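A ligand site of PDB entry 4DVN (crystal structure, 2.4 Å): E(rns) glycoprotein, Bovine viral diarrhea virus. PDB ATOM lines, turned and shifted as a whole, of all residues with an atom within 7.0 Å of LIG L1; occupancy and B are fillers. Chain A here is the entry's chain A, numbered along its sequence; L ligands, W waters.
Water W5 lies within hydrogen-bond range of an oxygen (O6) of LG2 L2 (2.6 Å), an oxygen (O9) of LIG L1 (2.6 Å) and the side-chain amide nitrogen (NE2) of Gln 129 (2.9 Å).
Water W6 bridges an oxygen (O9) of LIG L1 (2.7 Å) and an oxygen (O6) of LG2 L2 (3.3 Å).
Water W2 lies within hydrogen-bond range of an oxygen (O1) of LIG L1 (2.8 Å) and the side-chain amide nitrogen (NE2) of Gln 7 (3.1 Å).
Water W8 bridges N2 of LIG L1 (2.8 Å) and O of Pro 36 (3.1 Å).
Residues that only touch LIG L1: Ile 5, Ile 39 and Arg 131.
Along chain A the residues within 4 Å of LIG L1 span positions 5 to 131.
NE2 of His 81 lies close to NE1 of Trp 35, 3.4 Å away.
The side-chain amide oxygen (OE1) of Gln 129 lies within hydrogen-bond range of a ring nitrogen (ND1) of His 32 (2.8 Å).
O of Gln 7 lies within hydrogen-bond range of N of His 32 (2.9 Å).
OE2 of Glu 77 lies close to NE2 of His 32, 3.5 Å away.
O of Ile 5 is in hydrogen-bond range of N of Trp 35 (2.7 Å).
The side-chain carboxylate (OE1) of Glu 77 sits at hydrogen-bond distance from the indole nitrogen (NE1) of Trp 35.
The side-chain amide oxygen (OE1) of Gln 7 sits at hydrogen-bond distance from the guanidinium group (NH2) of Arg 131 (2.9 Å).
The indole nitrogen (NE1) of Trp 35 sits close to an oxygen (O7) of LIG L1 (3.4 Å).
O7 of LIG L1 lies within hydrogen-bond range of NE2 of His 32, at 3.3 Å.
An oxygen (O3) of LG2 L2 sits at hydrogen-bond distance from a ring nitrogen (ND1) of His 32 (3.2 Å).
O6 of LIG L1 sits at hydrogen-bond distance from NE2 of His 81, at 2.6 Å.
OE2 of Glu 77 sits close to O7 of LIG L1.
NE2 of His 76 lies within hydrogen-bond range of O8 of LIG L1 (2.6 Å).
An oxygen (O6) of LG2 L2 lies within hydrogen-bond range of the side-chain amide nitrogen (NE2) of Gln 129 (3.4 Å).
NZ of Lys 80 is in salt-bridge range of O6 of LIG L1 (2.8 Å).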
ATOM      1  N   ILE A   5      22.540 -19.922  -9.250  1.00  0.00           N
ATOM      2  CA  ILE A   5      22.132 -18.550  -8.923  1.00  0.00           C
ATOM      3  C   ILE A   5      20.857 -18.204  -9.677  1.00  0.00           C
ATOM      4  O   ILE A   5      20.840 -18.275 -10.907  1.00  0.00           O
ATOM      5  CB  ILE A   5      23.262 -17.531  -9.240  1.00  0.00           C
ATOM      6  CG1 ILE A   5      24.519 -17.761  -8.378  1.00  0.00           C
ATOM      7  CG2 ILE A   5      22.755 -16.079  -9.086  1.00  0.00           C
ATOM      8  CD1 ILE A   5      25.773 -17.153  -8.919  1.00  0.00           C
ATOM      9  N   GLN A   7      18.573 -15.130 -10.645  1.00  0.00           N
ATOM     10  CA  GLN A   7      18.553 -13.674 -10.710  1.00  0.00           C
ATOM     11  C   GLN A   7      17.339 -13.188 -11.483  1.00  0.00           C
ATOM     12  O   GLN A   7      16.910 -13.858 -12.422  1.00  0.00           O
ATOM     13  CB  GLN A   7      19.856 -13.134 -11.329  1.00  0.00           C
ATOM     14  CG  GLN A   7      19.998 -11.622 -11.160  1.00  0.00           C
ATOM     15  CD  GLN A   7      21.410 -11.132 -11.171  1.00  0.00           C
ATOM     16  OE1 GLN A   7      22.245 -11.563 -10.380  1.00  0.00           O
ATOM     17  NE2 GLN A   7      21.699 -10.184 -12.043  1.00  0.00           N
ATOM     18  N   HIS A  32      15.523 -13.310 -14.852  1.00  0.00           N
ATOM     19  CA  HIS A  32      16.634 -13.014 -15.750  1.00  0.00           C
ATOM     20  C   HIS A  32      17.232 -14.365 -16.157  1.00  0.00           C
ATOM     21  O   HIS A  32      17.238 -14.699 -17.342  1.00  0.00           O
ATOM     22  CB  HIS A  32      17.667 -12.069 -15.105  1.00  0.00           C
ATOM     23  CG  HIS A  32      18.815 -11.713 -16.004  1.00  0.00           C
ATOM     24  ND1 HIS A  32      19.681 -10.670 -15.679  1.00  0.00           N
ATOM     25  CD2 HIS A  32      19.211 -12.253 -17.196  1.00  0.00           C
ATOM     26  CE1 HIS A  32      20.566 -10.637 -16.661  1.00  0.00           C
ATOM     27  NE2 HIS A  32      20.325 -11.570 -17.591  1.00  0.00           N
ATOM     28  N   GLY A  33      17.655 -15.160 -15.167  1.00  0.00           N
ATOM     29  CA  GLY A  33      18.197 -16.488 -15.400  1.00  0.00           C
ATOM     30  C   GLY A  33      18.427 -17.332 -14.173  1.00  0.00           C
ATOM     31  O   GLY A  33      18.300 -16.853 -13.047  1.00  0.00           O
ATOM     32  N   TRP A  35      21.448 -19.744 -13.053  1.00  0.00           N
ATOM     33  CA  TRP A  35      22.828 -19.957 -13.425  1.00  0.00           C
ATOM     34  C   TRP A  35      23.659 -20.986 -12.693  1.00  0.00           C
ATOM     35  O   TRP A  35      24.319 -20.622 -11.724  1.00  0.00           O
ATOM     36  CB  TRP A  35      23.590 -18.602 -13.526  1.00  0.00           C
ATOM     37  CG  TRP A  35      22.873 -17.523 -14.297  1.00  0.00           C
ATOM     38  CD1 TRP A  35      22.210 -17.656 -15.484  1.00  0.00           C
ATOM     39  CD2 TRP A  35      22.845 -16.116 -13.985  1.00  0.00           C
ATOM     40  NE1 TRP A  35      21.749 -16.427 -15.913  1.00  0.00           N
ATOM     41  CE2 TRP A  35      22.130 -15.465 -15.010  1.00  0.00           C
ATOM     42  CE3 TRP A  35      23.340 -15.344 -12.905  1.00  0.00           C
ATOM     43  CZ2 TRP A  35      21.892 -14.081 -14.988  1.00  0.00           C
ATOM     44  CZ3 TRP A  35      23.143 -13.960 -12.896  1.00  0.00           C
ATOM     45  CH2 TRP A  35      22.414 -13.349 -13.919  1.00  0.00           C
ATOM     46  N   PRO A  36      23.809 -22.233 -13.252  1.00  0.00           N
ATOM     47  CA  PRO A  36      24.795 -23.186 -12.684  1.00  0.00           C
ATOM     48  C   PRO A  36      26.222 -22.693 -12.981  1.00  0.00           C
ATOM     49  O   PRO A  36      26.406 -21.738 -13.738  1.00  0.00           O
ATOM     50  CB  PRO A  36      24.519 -24.486 -13.467  1.00  0.00           C
ATOM     51  CG  PRO A  36      23.218 -24.285 -14.116  1.00  0.00           C
ATOM     52  CD  PRO A  36      23.143 -22.838 -14.425  1.00  0.00           C
ATOM     53  N   GLU A  37      27.239 -23.328 -12.384  1.00  0.00           N
ATOM     54  CA  GLU A  37      28.657 -22.981 -12.545  1.00  0.00           C
ATOM     55  C   GLU A  37      29.087 -23.038 -14.004  1.00  0.00           C
ATOM     56  O   GLU A  37      29.763 -22.124 -14.473  1.00  0.00           O
ATOM     57  CB  GLU A  37      29.531 -23.945 -11.720  1.00  0.00           C
ATOM     58  CG  GLU A  37      30.706 -23.306 -11.002  1.00  0.00           C
ATOM     59  CD  GLU A  37      30.382 -22.624  -9.677  1.00  0.00           C
ATOM     60  OE1 GLU A  37      29.512 -23.117  -8.932  1.00  0.00           O
ATOM     61  OE2 GLU A  37      31.033 -21.597  -9.375  1.00  0.00           O
ATOM     62  N   ILE A  39      29.040 -22.723 -17.854  1.00  0.00           N
ATOM     63  CA  ILE A  39      28.539 -21.902 -18.952  1.00  0.00           C
ATOM     64  C   ILE A  39      28.699 -22.724 -20.234  1.00  0.00           C
ATOM     65  O   ILE A  39      29.749 -23.329 -20.477  1.00  0.00           O
ATOM     66  CB  ILE A  39      29.206 -20.498 -18.999  1.00  0.00           C
ATOM     67  CG1 ILE A  39      28.537 -19.567 -17.946  1.00  0.00           C
ATOM     68  CG2 ILE A  39      29.110 -19.878 -20.413  1.00  0.00           C
ATOM     69  CD1 ILE A  39      29.069 -18.116 -17.881  1.00  0.00           C
ATOM     70  N   LEU A  73      16.069 -12.598 -24.664  1.00  0.00           N
ATOM     71  CA  LEU A  73      16.695 -12.940 -23.380  1.00  0.00           C
ATOM     72  C   LEU A  73      16.532 -14.443 -23.096  1.00  0.00           C
ATOM     73  O   LEU A  73      17.509 -15.105 -22.748  1.00  0.00           O
ATOM     74  CB  LEU A  73      16.140 -12.066 -22.224  1.00  0.00           C
ATOM     75  CG  LEU A  73      16.698 -12.332 -20.803  1.00  0.00           C
ATOM     76  CD1 LEU A  73      18.248 -12.139 -20.731  1.00  0.00           C
ATOM     77  CD2 LEU A  73      15.993 -11.459 -19.793  1.00  0.00           C
ATOM     78  N   HIS A  76      18.817 -16.554 -25.306  1.00  0.00           N
ATOM     79  CA  HIS A  76      20.182 -16.307 -24.832  1.00  0.00           C
ATOM     80  C   HIS A  76      20.466 -17.113 -23.576  1.00  0.00           C
ATOM     81  O   HIS A  76      21.560 -17.656 -23.444  1.00  0.00           O
ATOM     82  CB  HIS A  76      20.390 -14.791 -24.572  1.00  0.00           C
ATOM     83  CG  HIS A  76      21.602 -14.488 -23.758  1.00  0.00           C
ATOM     84  ND1 HIS A  76      22.864 -14.460 -24.317  1.00  0.00           N
ATOM     85  CD2 HIS A  76      21.709 -14.253 -22.428  1.00  0.00           C
ATOM     86  CE1 HIS A  76      23.689 -14.190 -23.322  1.00  0.00           C
ATOM     87  NE2 HIS A  76      23.036 -14.055 -22.167  1.00  0.00           N
ATOM     88  N   GLU A  77      19.478 -17.212 -22.662  1.00  0.00           N
ATOM     89  CA  GLU A  77      19.589 -17.964 -21.415  1.00  0.00           C
ATOM     90  C   GLU A  77      19.654 -19.455 -21.655  1.00  0.00           C
ATOM     91  O   GLU A  77      20.424 -20.130 -20.975  1.00  0.00           O
ATOM     92  CB  GLU A  77      18.464 -17.613 -20.441  1.00  0.00           C
ATOM     93  CG  GLU A  77      18.558 -16.188 -19.906  1.00  0.00           C
ATOM     94  CD  GLU A  77      19.804 -15.814 -19.128  1.00  0.00           C
ATOM     95  OE1 GLU A  77      20.306 -16.659 -18.358  1.00  0.00           O
ATOM     96  OE2 GLU A  77      20.236 -14.653 -19.240  1.00  0.00           O
ATOM     97  N   LYS A  80      23.329 -20.047 -23.428  1.00  0.00           N
ATOM     98  CA  LYS A  80      24.454 -19.797 -22.515  1.00  0.00           C
ATOM     99  C   LYS A  80      24.419 -20.619 -21.233  1.00  0.00           C
ATOM    100  O   LYS A  80      25.483 -20.989 -20.726  1.00  0.00           O
ATOM    101  CB  LYS A  80      24.540 -18.282 -22.195  1.00  0.00           C
ATOM    102  CG  LYS A  80      25.842 -17.832 -21.542  1.00  0.00           C
ATOM    103  CD  LYS A  80      25.825 -16.343 -21.265  1.00  0.00           C
ATOM    104  CE  LYS A  80      27.096 -15.884 -20.594  1.00  0.00           C
ATOM    105  NZ  LYS A  80      27.018 -14.463 -20.138  1.00  0.00           N
ATOM    106  N   HIS A  81      23.216 -20.907 -20.677  1.00  0.00           N
ATOM    107  CA  HIS A  81      23.107 -21.598 -19.395  1.00  0.00           C
ATOM    108  C   HIS A  81      22.241 -22.849 -19.344  1.00  0.00           C
ATOM    109  O   HIS A  81      22.293 -23.578 -18.353  1.00  0.00           O
ATOM    110  CB  HIS A  81      22.559 -20.619 -18.333  1.00  0.00           C
ATOM    111  CG  HIS A  81      23.338 -19.345 -18.214  1.00  0.00           C
ATOM    112  ND1 HIS A  81      24.522 -19.286 -17.514  1.00  0.00           N
ATOM    113  CD2 HIS A  81      23.066 -18.125 -18.725  1.00  0.00           C
ATOM    114  CE1 HIS A  81      24.914 -18.037 -17.587  1.00  0.00           C
ATOM    115  NE2 HIS A  81      24.074 -17.300 -18.301  1.00  0.00           N
ATOM    116  N   VAL A 114      21.403  -6.779  -6.316  1.00  0.00           N
ATOM    117  CA  VAL A 114      22.542  -6.994  -7.197  1.00  0.00           C
ATOM    118  C   VAL A 114      22.970  -5.615  -7.697  1.00  0.00           C
ATOM    119  O   VAL A 114      24.091  -5.183  -7.456  1.00  0.00           O
ATOM    120  CB  VAL A 114      22.240  -8.016  -8.344  1.00  0.00           C
ATOM    121  CG1 VAL A 114      23.401  -8.086  -9.343  1.00  0.00           C
ATOM    122  CG2 VAL A 114      21.927  -9.390  -7.783  1.00  0.00           C
ATOM    123  N   GLN A 129      17.934  -5.216 -10.041  1.00  0.00           N
ATOM    124  CA  GLN A 129      18.182  -6.655 -10.194  1.00  0.00           C
ATOM    125  C   GLN A 129      18.490  -7.236  -8.815  1.00  0.00           C
ATOM    126  O   GLN A 129      19.225  -6.624  -8.034  1.00  0.00           O
ATOM    127  CB  GLN A 129      19.352  -6.947 -11.142  1.00  0.00           C
ATOM    128  CG  GLN A 129      19.044  -6.712 -12.614  1.00  0.00           C
ATOM    129  CD  GLN A 129      19.851  -7.581 -13.537  1.00  0.00           C
ATOM    130  OE1 GLN A 129      19.646  -8.804 -13.648  1.00  0.00           O
ATOM    131  NE2 GLN A 129      20.763  -6.969 -14.266  1.00  0.00           N
ATOM    132  N   ARG A 131      18.875 -11.296  -6.530  1.00  0.00           N
ATOM    133  CA  ARG A 131      19.153 -12.728  -6.611  1.00  0.00           C
ATOM    134  C   ARG A 131      18.851 -13.418  -5.283  1.00  0.00           C
ATOM    135  O   ARG A 131      18.600 -12.751  -4.293  1.00  0.00           O
ATOM    136  CB  ARG A 131      20.579 -13.006  -7.119  1.00  0.00           C
ATOM    137  CG  ARG A 131      21.681 -12.536  -6.186  1.00  0.00           C
ATOM    138  CD  ARG A 131      23.025 -13.098  -6.602  1.00  0.00           C
ATOM    139  NE  ARG A 131      23.440 -12.620  -7.924  1.00  0.00           N
ATOM    140  CZ  ARG A 131      24.593 -12.950  -8.497  1.00  0.00           C
ATOM    141  NH1 ARG A 131      25.447 -13.745  -7.858  1.00  0.00           N
ATOM    142  NH2 ARG A 131      24.898 -12.497  -9.697  1.00  0.00           N
HETATM  143  O1  LIG L   1      26.686 -10.290 -13.699  1.00  0.00           O
HETATM  144  C1  LIG L   1      26.605  -9.726 -14.994  1.00  0.00           C
HETATM  145  C2  LIG L   1      26.104 -10.762 -15.997  1.00  0.00           C
HETATM  146  O2  LIG L   1      26.989 -11.888 -15.964  1.00  0.00           O
HETATM  147  C3  LIG L   1      26.269 -13.152 -16.108  1.00  0.00           C
HETATM  148  N1  LIG L   1      26.450 -14.063 -14.921  1.00  0.00           N
HETATM  149  C4  LIG L   1      26.534 -13.556 -13.615  1.00  0.00           C
HETATM  150  C5  LIG L   1      26.700 -14.382 -12.523  1.00  0.00           C
HETATM  151  C6  LIG L   1      26.784 -15.804 -12.751  1.00  0.00           C
HETATM  152  O3  LIG L   1      26.912 -16.612 -11.802  1.00  0.00           O
HETATM  153  N2  LIG L   1      26.695 -16.251 -14.045  1.00  0.00           N
HETATM  154  C7  LIG L   1      26.543 -15.417 -15.119  1.00  0.00           C
HETATM  155  O4  LIG L   1      26.505 -15.892 -16.252  1.00  0.00           O
HETATM  156  C8  LIG L   1      24.781 -12.757 -16.361  1.00  0.00           C
HETATM  157  O5  LIG L   1      24.593 -12.489 -17.713  1.00  0.00           O
HETATM  158  P1  LIG L   1      24.012 -13.659 -18.616  1.00  0.00           P
HETATM  159  O6  LIG L   1      24.819 -14.857 -18.525  1.00  0.00           O
HETATM  160  O7  LIG L   1      22.493 -13.994 -18.238  1.00  0.00           O
HETATM  161  O8  LIG L   1      23.979 -12.999 -20.041  1.00  0.00           O
HETATM  162  C9  LIG L   1      24.703 -11.337 -15.668  1.00  0.00           C
HETATM  163  O9  LIG L   1      23.620 -10.476 -16.166  1.00  0.00           O
HETATM  164  O1  LG2 L   2      20.508  -4.081 -23.067  1.00  0.00           O
HETATM  165  C1  LG2 L   2      21.219  -4.558 -21.913  1.00  0.00           C
HETATM  166  C2  LG2 L   2      21.156  -3.498 -20.820  1.00  0.00           C
HETATM  167  O2  LG2 L   2      20.142  -3.769 -19.847  1.00  0.00           O
HETATM  168  C3  LG2 L   2      20.748  -4.356 -18.651  1.00  0.00           C
HETATM  169  N1  LG2 L   2      19.990  -5.627 -18.420  1.00  0.00           N
HETATM  170  C4  LG2 L   2      20.158  -6.699 -19.301  1.00  0.00           C
HETATM  171  C5  LG2 L   2      19.479  -7.879 -19.128  1.00  0.00           C
HETATM  172  C6  LG2 L   2      18.564  -7.988 -18.029  1.00  0.00           C
HETATM  173  O3  LG2 L   2      17.945  -9.018 -17.852  1.00  0.00           O
HETATM  174  N2  LG2 L   2      18.401  -6.933 -17.203  1.00  0.00           N
HETATM  175  C7  LG2 L   2      19.103  -5.784 -17.378  1.00  0.00           C
HETATM  176  O4  LG2 L   2      18.907  -4.898 -16.587  1.00  0.00           O
HETATM  177  C8  LG2 L   2      22.277  -4.484 -18.976  1.00  0.00           C
HETATM  178  O5  LG2 L   2      23.121  -4.190 -17.845  1.00  0.00           O
HETATM  179  P1  LG2 L   2      23.652  -5.572 -17.172  1.00  0.00           P
HETATM  180  O6  LG2 L   2      22.557  -6.571 -17.095  1.00  0.00           O
HETATM  181  O7  LG2 L   2      24.842  -6.209 -18.055  1.00  0.00           O
HETATM  182  O8  LG2 L   2      24.083  -5.263 -15.614  1.00  0.00           O
HETATM  183  C9  LG2 L   2      22.473  -3.423 -20.073  1.00  0.00           C
HETATM  184  O9  LG2 L   2      22.573  -2.131 -19.494  1.00  0.00           O
HETATM  185  O   HOH W   1      25.631 -11.061 -20.681  1.00  0.00           O
HETATM  186  O   HOH W   2      24.523  -8.962 -12.518  1.00  0.00           O
HETATM  187  O   HOH W   3      26.986 -19.915 -10.811  1.00  0.00           O
HETATM  188  O   HOH W   4      29.851 -14.143 -15.372  1.00  0.00           O
HETATM  189  O   HOH W   5      23.246  -8.108 -15.115  1.00  0.00           O
HETATM  190  O   HOH W   6      23.612  -9.277 -18.616  1.00  0.00           O
HETATM  191  O   HOH W   7      27.004  -9.325 -11.158  1.00  0.00           O
HETATM  192  O   HOH W   8      27.374 -18.925 -14.667  1.00  0.00           O
